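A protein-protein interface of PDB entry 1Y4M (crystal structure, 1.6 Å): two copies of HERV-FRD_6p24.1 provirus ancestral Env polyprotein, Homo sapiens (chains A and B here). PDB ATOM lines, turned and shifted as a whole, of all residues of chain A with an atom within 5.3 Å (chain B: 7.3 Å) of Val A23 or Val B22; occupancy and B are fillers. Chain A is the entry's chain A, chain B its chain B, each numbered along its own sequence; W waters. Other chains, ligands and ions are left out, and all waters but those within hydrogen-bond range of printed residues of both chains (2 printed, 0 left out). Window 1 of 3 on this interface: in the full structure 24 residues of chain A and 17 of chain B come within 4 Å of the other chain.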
ATOM      1  N   LEU A  19     -24.509   1.904  -0.911  1.00  0.00           N
ATOM      2  CA  LEU A  19     -24.292   0.703  -1.701  1.00  0.00           C
ATOM      3  C   LEU A  19     -24.704   0.945  -3.143  1.00  0.00           C
ATOM      4  O   LEU A  19     -23.976   0.597  -4.072  1.00  0.00           O
ATOM      5  CB  LEU A  19     -25.091  -0.458  -1.119  1.00  0.00           C
ATOM      6  CG  LEU A  19     -24.643  -1.838  -1.601  1.00  0.00           C
ATOM      7  CD1 LEU A  19     -23.181  -2.055  -1.225  1.00  0.00           C
ATOM      8  CD2 LEU A  19     -25.522  -2.903  -0.964  1.00  0.00           C
ATOM      9  N   ALA A  20     -25.870   1.549  -3.335  1.00  0.00           N
ATOM     10  CA  ALA A  20     -26.331   1.824  -4.686  1.00  0.00           C
ATOM     11  C   ALA A  20     -25.279   2.619  -5.453  1.00  0.00           C
ATOM     12  O   ALA A  20     -25.077   2.397  -6.639  1.00  0.00           O
ATOM     13  CB  ALA A  20     -27.644   2.583  -4.650  1.00  0.00           C
ATOM     14  N   ALA A  21     -24.604   3.542  -4.774  1.00  0.00           N
ATOM     15  CA  ALA A  21     -23.577   4.353  -5.420  1.00  0.00           C
ATOM     16  C   ALA A  21     -22.473   3.458  -5.954  1.00  0.00           C
ATOM     17  O   ALA A  21     -22.001   3.631  -7.074  1.00  0.00           O
ATOM     18  CB  ALA A  21     -22.989   5.356  -4.428  1.00  0.00           C
ATOM     19  N   VAL A  22     -22.055   2.508  -5.131  1.00  0.00           N
ATOM     20  CA  VAL A  22     -21.009   1.586  -5.528  1.00  0.00           C
ATOM     21  C   VAL A  22     -21.510   0.711  -6.663  1.00  0.00           C
ATOM     22  O   VAL A  22     -20.811   0.497  -7.658  1.00  0.00           O
ATOM     23  CB  VAL A  22     -20.600   0.684  -4.364  1.00  0.00           C
ATOM     24  CG1 VAL A  22     -19.448  -0.215  -4.783  1.00  0.00           C
ATOM     25  CG2 VAL A  22     -20.214   1.538  -3.172  1.00  0.00           C
ATOM     26  N   VAL A  23     -22.725   0.209  -6.508  1.00  0.00           N
ATOM     27  CA  VAL A  23     -23.318  -0.653  -7.523  1.00  0.00           C
ATOM     28  C   VAL A  23     -23.422   0.060  -8.861  1.00  0.00           C
ATOM     29  O   VAL A  23     -23.064  -0.496  -9.903  1.00  0.00           O
ATOM     30  CB  VAL A  23     -24.711  -1.132  -7.091  1.00  0.00           C
ATOM     31  CG1 VAL A  23     -25.338  -1.959  -8.197  1.00  0.00           C
ATOM     32  CG2 VAL A  23     -24.594  -1.943  -5.817  1.00  0.00           C
ATOM     33  N   LEU A  24     -23.908   1.294  -8.838  1.00  0.00           N
ATOM     34  CA  LEU A  24     -24.045   2.054 -10.070  1.00  0.00           C
ATOM     35  C   LEU A  24     -22.687   2.328 -10.686  1.00  0.00           C
ATOM     36  O   LEU A  24     -22.532   2.280 -11.903  1.00  0.00           O
ATOM     37  CB  LEU A  24     -24.764   3.371  -9.798  1.00  0.00           C
ATOM     38  CG  LEU A  24     -26.256   3.236  -9.500  1.00  0.00           C
ATOM     39  CD1 LEU A  24     -26.794   4.575  -9.037  1.00  0.00           C
ATOM     40  CD2 LEU A  24     -26.997   2.749 -10.739  1.00  0.00           C
ATOM     41  N   GLN A  25     -21.704   2.625  -9.847  1.00  0.00           N
ATOM     42  CA  GLN A  25     -20.372   2.895 -10.349  1.00  0.00           C
ATOM     43  C   GLN A  25     -19.809   1.609 -10.941  1.00  0.00           C
ATOM     44  O   GLN A  25     -19.112   1.631 -11.947  1.00  0.00           O
ATOM     45  CB  GLN A  25     -19.473   3.404  -9.226  1.00  0.00           C
ATOM     46  CG  GLN A  25     -18.116   3.847  -9.706  1.00  0.00           C
ATOM     47  CD  GLN A  25     -17.408   4.688  -8.679  1.00  0.00           C
ATOM     48  OE1 GLN A  25     -16.974   5.806  -8.969  1.00  0.00           O
ATOM     49  NE2 GLN A  25     -17.285   4.161  -7.467  1.00  0.00           N
ATOM     50  N   ASN A  26     -20.135   0.482 -10.321  1.00  0.00           N
ATOM     51  CA  ASN A  26     -19.667  -0.787 -10.831  1.00  0.00           C
ATOM     52  C   ASN A  26     -20.316  -1.037 -12.162  1.00  0.00           C
ATOM     53  O   ASN A  26     -19.699  -1.573 -13.072  1.00  0.00           O
ATOM     54  CB  ASN A  26     -20.034  -1.926  -9.901  1.00  0.00           C
ATOM     55  CG  ASN A  26     -19.177  -1.955  -8.682  1.00  0.00           C
ATOM     56  OD1 ASN A  26     -18.129  -1.333  -8.652  1.00  0.00           O
ATOM     57  ND2 ASN A  26     -19.602  -2.694  -7.672  1.00  0.00           N
ATOM     58  N   ARG A  27     -21.578  -0.656 -12.271  1.00  0.00           N
ATOM     59  CA  ARG A  27     -22.286  -0.871 -13.516  1.00  0.00           C
ATOM     60  C   ARG A  27     -21.651  -0.026 -14.603  1.00  0.00           C
ATOM     61  O   ARG A  27     -21.488  -0.483 -15.721  1.00  0.00           O
ATOM     62  CB  ARG A  27     -23.761  -0.506 -13.365  1.00  0.00           C
ATOM     63  CG  ARG A  27     -24.508  -0.488 -14.684  1.00  0.00           C
ATOM     64  CD  ARG A  27     -24.349  -1.803 -15.431  1.00  0.00           C
ATOM     65  NE  ARG A  27     -24.923  -2.927 -14.704  1.00  0.00           N
ATOM     66  CZ  ARG A  27     -26.203  -3.281 -14.755  1.00  0.00           C
ATOM     67  NH1 ARG A  27     -27.055  -2.599 -15.512  1.00  0.00           N
ATOM     68  NH2 ARG A  27     -26.637  -4.310 -14.038  1.00  0.00           N
ATOM     69  N   ARG A  28     -21.304   1.213 -14.271  1.00  0.00           N
ATOM     70  CA  ARG A  28     -20.677   2.083 -15.248  1.00  0.00           C
ATOM     71  C   ARG A  28     -19.359   1.445 -15.652  1.00  0.00           C
ATOM     72  O   ARG A  28     -18.992   1.448 -16.825  1.00  0.00           O
ATOM     73  CB  ARG A  28     -20.449   3.475 -14.655  1.00  0.00           C
ATOM     74  CG  ARG A  28     -21.752   4.220 -14.372  1.00  0.00           C
ATOM     75  CD  ARG A  28     -21.523   5.707 -14.168  1.00  0.00           C
ATOM     76  NE  ARG A  28     -20.838   6.009 -12.913  1.00  0.00           N
ATOM     77  CZ  ARG A  28     -21.402   5.924 -11.713  1.00  0.00           C
ATOM     78  NH1 ARG A  28     -20.700   6.223 -10.626  1.00  0.00           N
ATOM     79  NH2 ARG A  28     -22.667   5.544 -11.597  1.00  0.00           N
ATOM     80  N   CYS A  49     -30.926  -4.271 -15.786  1.00  0.00           N
ATOM     81  CA  CYS A  49     -31.466  -4.054 -14.451  1.00  0.00           C
ATOM     82  C   CYS A  49     -31.020  -2.669 -14.042  1.00  0.00           C
ATOM     83  O   CYS A  49     -29.867  -2.300 -14.253  1.00  0.00           O
ATOM     84  CB  CYS A  49     -30.908  -5.071 -13.460  1.00  0.00           C
ATOM     85  SG  CYS A  49     -31.458  -6.748 -13.762  1.00  0.00           S
ATOM     86  N   PHE A  50     -31.935  -1.907 -13.451  1.00  0.00           N
ATOM     87  CA  PHE A  50     -31.641  -0.545 -13.027  1.00  0.00           C
ATOM     88  C   PHE A  50     -31.960  -0.286 -11.559  1.00  0.00           C
ATOM     89  O   PHE A  50     -32.643  -1.070 -10.907  1.00  0.00           O
ATOM     90  CB  PHE A  50     -32.437   0.438 -13.881  1.00  0.00           C
ATOM     91  CG  PHE A  50     -32.172   0.320 -15.349  1.00  0.00           C
ATOM     92  CD1 PHE A  50     -31.111   1.000 -15.936  1.00  0.00           C
ATOM     93  CD2 PHE A  50     -32.980  -0.480 -16.145  1.00  0.00           C
ATOM     94  CE1 PHE A  50     -30.861   0.887 -17.303  1.00  0.00           C
ATOM     95  CE2 PHE A  50     -32.739  -0.600 -17.509  1.00  0.00           C
ATOM     96  CZ  PHE A  50     -31.677   0.085 -18.089  1.00  0.00           C
ATOM     97  N   TRP A  51     -31.454   0.840 -11.068  1.00  0.00           N
ATOM     98  CA  TRP A  51     -31.654   1.302  -9.697  1.00  0.00           C
ATOM     99  C   TRP A  51     -33.003   2.035  -9.637  1.00  0.00           C
ATOM    100  O   TRP A  51     -33.540   2.432 -10.672  1.00  0.00           O
ATOM    101  CB  TRP A  51     -30.511   2.258  -9.339  1.00  0.00           C
ATOM    102  CG  TRP A  51     -30.591   2.934  -8.002  1.00  0.00           C
ATOM    103  CD1 TRP A  51     -30.230   4.221  -7.722  1.00  0.00           C
ATOM    104  CD2 TRP A  51     -30.990   2.352  -6.756  1.00  0.00           C
ATOM    105  NE1 TRP A  51     -30.376   4.479  -6.382  1.00  0.00           N
ATOM    106  CE2 TRP A  51     -30.842   3.348  -5.763  1.00  0.00           C
ATOM    107  CE3 TRP A  51     -31.458   1.088  -6.379  1.00  0.00           C
ATOM    108  CZ2 TRP A  51     -31.145   3.121  -4.418  1.00  0.00           C
ATOM    109  CZ3 TRP A  51     -31.759   0.859  -5.041  1.00  0.00           C
ATOM    110  CH2 TRP A  51     -31.600   1.874  -4.077  1.00  0.00           C
ATOM    111  N   ILE B  16     -33.819  -2.502  -2.167  1.00  0.00           N
ATOM    112  CA  ILE B  16     -32.906  -3.619  -1.996  1.00  0.00           C
ATOM    113  C   ILE B  16     -33.036  -4.607  -3.146  1.00  0.00           C
ATOM    114  O   ILE B  16     -32.043  -4.969  -3.774  1.00  0.00           O
ATOM    115  CB  ILE B  16     -33.176  -4.357  -0.680  1.00  0.00           C
ATOM    116  CG1 ILE B  16     -32.829  -3.441   0.496  1.00  0.00           C
ATOM    117  CG2 ILE B  16     -32.356  -5.641  -0.621  1.00  0.00           C
ATOM    118  CD1 ILE B  16     -33.236  -3.992   1.831  1.00  0.00           C
ATOM    119  N   ASP B  17     -34.258  -5.040  -3.430  1.00  0.00           N
ATOM    120  CA  ASP B  17     -34.458  -5.996  -4.507  1.00  0.00           C
ATOM    121  C   ASP B  17     -34.036  -5.443  -5.854  1.00  0.00           C
ATOM    122  O   ASP B  17     -33.466  -6.164  -6.667  1.00  0.00           O
ATOM    123  CB  ASP B  17     -35.912  -6.454  -4.561  1.00  0.00           C
ATOM    124  CG  ASP B  17     -36.208  -7.545  -3.555  1.00  0.00           C
ATOM    125  OD1 ASP B  17     -35.249  -8.040  -2.920  1.00  0.00           O
ATOM    126  OD2 ASP B  17     -37.394  -7.912  -3.401  1.00  0.00           O
ATOM    127  N   SER B  18     -34.317  -4.167  -6.094  1.00  0.00           N
ATOM    128  CA  SER B  18     -33.930  -3.549  -7.352  1.00  0.00           C
ATOM    129  C   SER B  18     -32.413  -3.515  -7.453  1.00  0.00           C
ATOM    130  O   SER B  18     -31.837  -3.888  -8.473  1.00  0.00           O
ATOM    131  CB  SER B  18     -34.471  -2.126  -7.436  1.00  0.00           C
ATOM    132  OG  SER B  18     -35.878  -2.113  -7.299  1.00  0.00           O
ATOM    133  N   LEU B  19     -31.766  -3.064  -6.386  1.00  0.00           N
ATOM    134  CA  LEU B  19     -30.315  -2.984  -6.378  1.00  0.00           C
ATOM    135  C   LEU B  19     -29.739  -4.378  -6.537  1.00  0.00           C
ATOM    136  O   LEU B  19     -28.802  -4.585  -7.299  1.00  0.00           O
ATOM    137  CB  LEU B  19     -29.819  -2.374  -5.063  1.00  0.00           C
ATOM    138  CG  LEU B  19     -28.337  -2.004  -5.006  1.00  0.00           C
ATOM    139  CD1 LEU B  19     -28.048  -0.893  -6.004  1.00  0.00           C
ATOM    140  CD2 LEU B  19     -27.976  -1.552  -3.599  1.00  0.00           C
ATOM    141  N   ALA B  20     -30.312  -5.334  -5.816  1.00  0.00           N
ATOM    142  CA  ALA B  20     -29.836  -6.705  -5.877  1.00  0.00           C
ATOM    143  C   ALA B  20     -29.822  -7.185  -7.318  1.00  0.00           C
ATOM    144  O   ALA B  20     -28.891  -7.860  -7.740  1.00  0.00           O
ATOM    145  CB  ALA B  20     -30.720  -7.595  -5.040  1.00  0.00           C
ATOM    146  N   ALA B  21     -30.850  -6.826  -8.077  1.00  0.00           N
ATOM    147  CA  ALA B  21     -30.917  -7.249  -9.473  1.00  0.00           C
ATOM    148  C   ALA B  21     -29.740  -6.682 -10.252  1.00  0.00           C
ATOM    149  O   ALA B  21     -29.125  -7.373 -11.063  1.00  0.00           O
ATOM    150  CB  ALA B  21     -32.226  -6.793 -10.101  1.00  0.00           C
ATOM    151  N   VAL B  22     -29.427  -5.415 -10.007  1.00  0.00           N
ATOM    152  CA  VAL B  22     -28.319  -4.775 -10.696  1.00  0.00           C
ATOM    153  C   VAL B  22     -27.021  -5.450 -10.284  1.00  0.00           C
ATOM    154  O   VAL B  22     -26.161  -5.739 -11.112  1.00  0.00           O
ATOM    155  CB  VAL B  22     -28.223  -3.284 -10.330  1.00  0.00           C
ATOM    156  CG1 VAL B  22     -27.072  -2.643 -11.079  1.00  0.00           C
ATOM    157  CG2 VAL B  22     -29.530  -2.587 -10.653  1.00  0.00           C
ATOM    158  N   VAL B  23     -26.893  -5.715  -8.991  1.00  0.00           N
ATOM    159  CA  VAL B  23     -25.690  -6.344  -8.474  1.00  0.00           C
ATOM    160  C   VAL B  23     -25.469  -7.727  -9.042  1.00  0.00           C
ATOM    161  O   VAL B  23     -24.361  -8.068  -9.445  1.00  0.00           O
ATOM    162  CB  VAL B  23     -25.744  -6.462  -6.955  1.00  0.00           C
ATOM    163  CG1 VAL B  23     -24.499  -7.170  -6.443  1.00  0.00           C
ATOM    164  CG2 VAL B  23     -25.860  -5.084  -6.350  1.00  0.00           C
ATOM    165  N   LEU B  24     -26.525  -8.528  -9.055  1.00  0.00           N
ATOM    166  CA  LEU B  24     -26.415  -9.877  -9.578  1.00  0.00           C
ATOM    167  C   LEU B  24     -26.072  -9.818 -11.054  1.00  0.00           C
ATOM    168  O   LEU B  24     -25.316 -10.646 -11.561  1.00  0.00           O
ATOM    169  CB  LEU B  24     -27.723 -10.633  -9.373  1.00  0.00           C
ATOM    170  CG  LEU B  24     -28.157 -10.812  -7.916  1.00  0.00           C
ATOM    171  CD1 LEU B  24     -29.496 -11.543  -7.878  1.00  0.00           C
ATOM    172  CD2 LEU B  24     -27.097 -11.585  -7.145  1.00  0.00           C
ATOM    173  N   GLN B  25     -26.622  -8.836 -11.748  1.00  0.00           N
ATOM    174  CA  GLN B  25     -26.339  -8.707 -13.165  1.00  0.00           C
ATOM    175  C   GLN B  25     -24.887  -8.295 -13.333  1.00  0.00           C
ATOM    176  O   GLN B  25     -24.195  -8.756 -14.232  1.00  0.00           O
ATOM    177  CB  GLN B  25     -27.269  -7.680 -13.788  1.00  0.00           C
ATOM    178  CG  GLN B  25     -27.030  -7.492 -15.255  1.00  0.00           C
ATOM    179  CD  GLN B  25     -28.168  -6.767 -15.902  1.00  0.00           C
ATOM    180  OE1 GLN B  25     -28.460  -5.624 -15.556  1.00  0.00           O
ATOM    181  NE2 GLN B  25     -28.836  -7.428 -16.836  1.00  0.00           N
ATOM    182  N   ASN B  26     -24.428  -7.410 -12.459  1.00  0.00           N
ATOM    183  CA  ASN B  26     -23.049  -6.984 -12.525  1.00  0.00           C
ATOM    184  C   ASN B  26     -22.172  -8.185 -12.270  1.00  0.00           C
ATOM    185  O   ASN B  26     -21.125  -8.330 -12.883  1.00  0.00           O
ATOM    186  CB  ASN B  26     -22.765  -5.934 -11.470  1.00  0.00           C
ATOM    187  CG  ASN B  26     -23.281  -4.580 -11.859  1.00  0.00           C
ATOM    188  OD1 ASN B  26     -23.780  -4.392 -12.969  1.00  0.00           O
ATOM    189  ND2 ASN B  26     -23.155  -3.615 -10.958  1.00  0.00           N
ATOM    190  N   ARG B  27     -22.608  -9.043 -11.358  1.00  0.00           N
ATOM    191  CA  ARG B  27     -21.844 -10.234 -11.061  1.00  0.00           C
ATOM    192  C   ARG B  27     -21.793 -11.143 -12.285  1.00  0.00           C
ATOM    193  O   ARG B  27     -20.741 -11.683 -12.592  1.00  0.00           O
ATOM    194  CB  ARG B  27     -22.431 -10.980  -9.865  1.00  0.00           C
ATOM    195  CG  ARG B  27     -21.824 -12.365  -9.670  1.00  0.00           C
ATOM    196  CD  ARG B  27     -20.310 -12.310  -9.578  1.00  0.00           C
ATOM    197  NE  ARG B  27     -19.879 -11.445  -8.484  1.00  0.00           N
ATOM    198  CZ  ARG B  27     -19.659 -11.868  -7.247  1.00  0.00           C
ATOM    199  NH1 ARG B  27     -19.822 -13.149  -6.946  1.00  0.00           N
ATOM    200  NH2 ARG B  27     -19.296 -11.011  -6.310  1.00  0.00           N
ATOM    201  N   ARG B  28     -22.912 -11.299 -12.990  1.00  0.00           N
ATOM    202  CA  ARG B  28     -22.902 -12.139 -14.182  1.00  0.00           C
ATOM    203  C   ARG B  28     -22.006 -11.509 -15.235  1.00  0.00           C
ATOM    204  O   ARG B  28     -21.325 -12.205 -15.989  1.00  0.00           O
ATOM    205  CB  ARG B  28     -24.313 -12.310 -14.737  1.00  0.00           C
ATOM    206  CG  ARG B  28     -25.229 -13.091 -13.819  1.00  0.00           C
ATOM    207  CD  ARG B  28     -26.512 -13.471 -14.545  1.00  0.00           C
ATOM    208  NE  ARG B  28     -27.324 -12.313 -14.865  1.00  0.00           N
ATOM    209  CZ  ARG B  28     -28.114 -11.690 -13.999  1.00  0.00           C
ATOM    210  NH1 ARG B  28     -28.200 -12.118 -12.747  1.00  0.00           N
ATOM    211  NH2 ARG B  28     -28.823 -10.639 -14.387  1.00  0.00           N
HETATM  212  O   HOH W   1     -30.257  -9.675 -12.112  1.00  0.00           O
HETATM  213  O   HOH W   2     -32.929  -3.775 -10.735  1.00  0.00           O
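Water W2 lies within hydrogen-bond range of the backbone carbonyl oxygen (O) of Ser B18 and the backbone carbonyl oxygen (O) of Phe A50.
Water W1 lies within hydrogen-bond range of the backbone carbonyl oxygen of Ala B21, the guanidinium group of Arg B28 and the side-chain sulfur of Cys A49.
O of Val A23 is in hydrogen-bond range of ND2 of Asn B26.
The guanidinium group of Arg A27 is in hydrogen-bond range of the backbone carbonyl oxygen of Val B22 (3.3 Å).
The side-chain amide oxygen (OE1) of Gln B25 sits at hydrogen-bond distance from the guanidinium group (NH2) of Arg A27 (2.7 Å).
OD1 of Asn B26 lies within hydrogen-bond range of NE of Arg A27, at 2.5 Å.
O of Ala B21 is in hydrogen-bond range of SG of Cys A49, at 3.6 Å.
The side-chain amide oxygen of Gln B25 is in hydrogen-bond range of the backbone NH of Cys A49 (2.8 Å).
OD1 of Asn A26 sits close to O of Val A22 (3.4 Å).
The guanidinium group of Arg A27 is in hydrogen-bond range of the backbone carbonyl oxygen of Cys A49 (3.1 Å).
The backbone carbonyl oxygen (O) of Val B22 sits close to the side-chain amide oxygen (OD1) of Asn B26 (3.3 Å).
Printed residues of chain B within 4 Å of Ala A20: Leu B19 (3.5 Å).
Val A23 touches four residues of chain B.
Of the printed residues of chain B, Cys A49 touches Ala B21, Val B22 and Gln B25.
Of the printed residues of chain A, Ser B18 touches Phe A50 (3.8 Å).
Of the printed residues of chain A, Val B22 touches Val A23, Arg A27, Cys A49, Phe A50 and Trp A51.
Printed residues of chain A within 4 Å of Val B23: Val A23.
The nearest residue of chain B that does not touch Val A23 is Ala B20 (6.5 Å).
The nearest printed residue of chain A that does not touch Val B22 is Leu A24 (5.4 Å).
The nearest printed residue of chain A that does not touch Ser B18 is Trp A51 (4.5 Å).
Leu A19 touches its own counterpart, Leu B19.
Val A23 touches Leu B19, but with the chains exchanged Leu A19 does not touch Val B23 (5.8 Å).
Asn A26 touches its own counterpart, Asn B26.
Arg A27 touches Val B22, but with the chains exchanged Val A22 does not touch Arg B27 (10.4 Å).
Among the printed residues, pairs that only touch across the chains: Val A23 with Val B23, Val A23 with Val B22, Phe A50 with Val B22, Ala A20 with Leu B19, Val A23 with Leu B19, Cys A49 with Val B22, Asn A26 with Asn B26, Trp A51 with Leu B19, Phe A50 with Ser B18, Leu A19 with Leu B19 and Trp A51 with Val B22.
Printed residues of chain B that touch a printed residue of chain A: Ser B18, Leu B19, Ala B21, Val B22, Val B23, Gln B25 and Asn B26.
Along chain B the printed residues that touch a printed residue of chain A span positions 18 to 26.
Of the 13 printed residues of chain A, 8 touch a printed residue of chain B.
Printed residues of chain A that touch a printed residue of chain B: Leu A19, Ala A20, Val A23, Asn A26, Arg A27, Cys A49, Phe A50 and Trp A51.
Hydrophobic or aromatic side chains of chain A within 4 Å of the printed part of chain B: Leu A19, Ala A20, Val A23 and Trp A51.
Along chain A the printed residues that touch a printed residue of chain B span positions 19 to 51.
Among the printed residues, 17 pairs touch across the chains.
Among the printed residues, no Asp or Glu carboxylate lies within 4 Å of a Lys or Arg side-chain nitrogen of the other chain.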
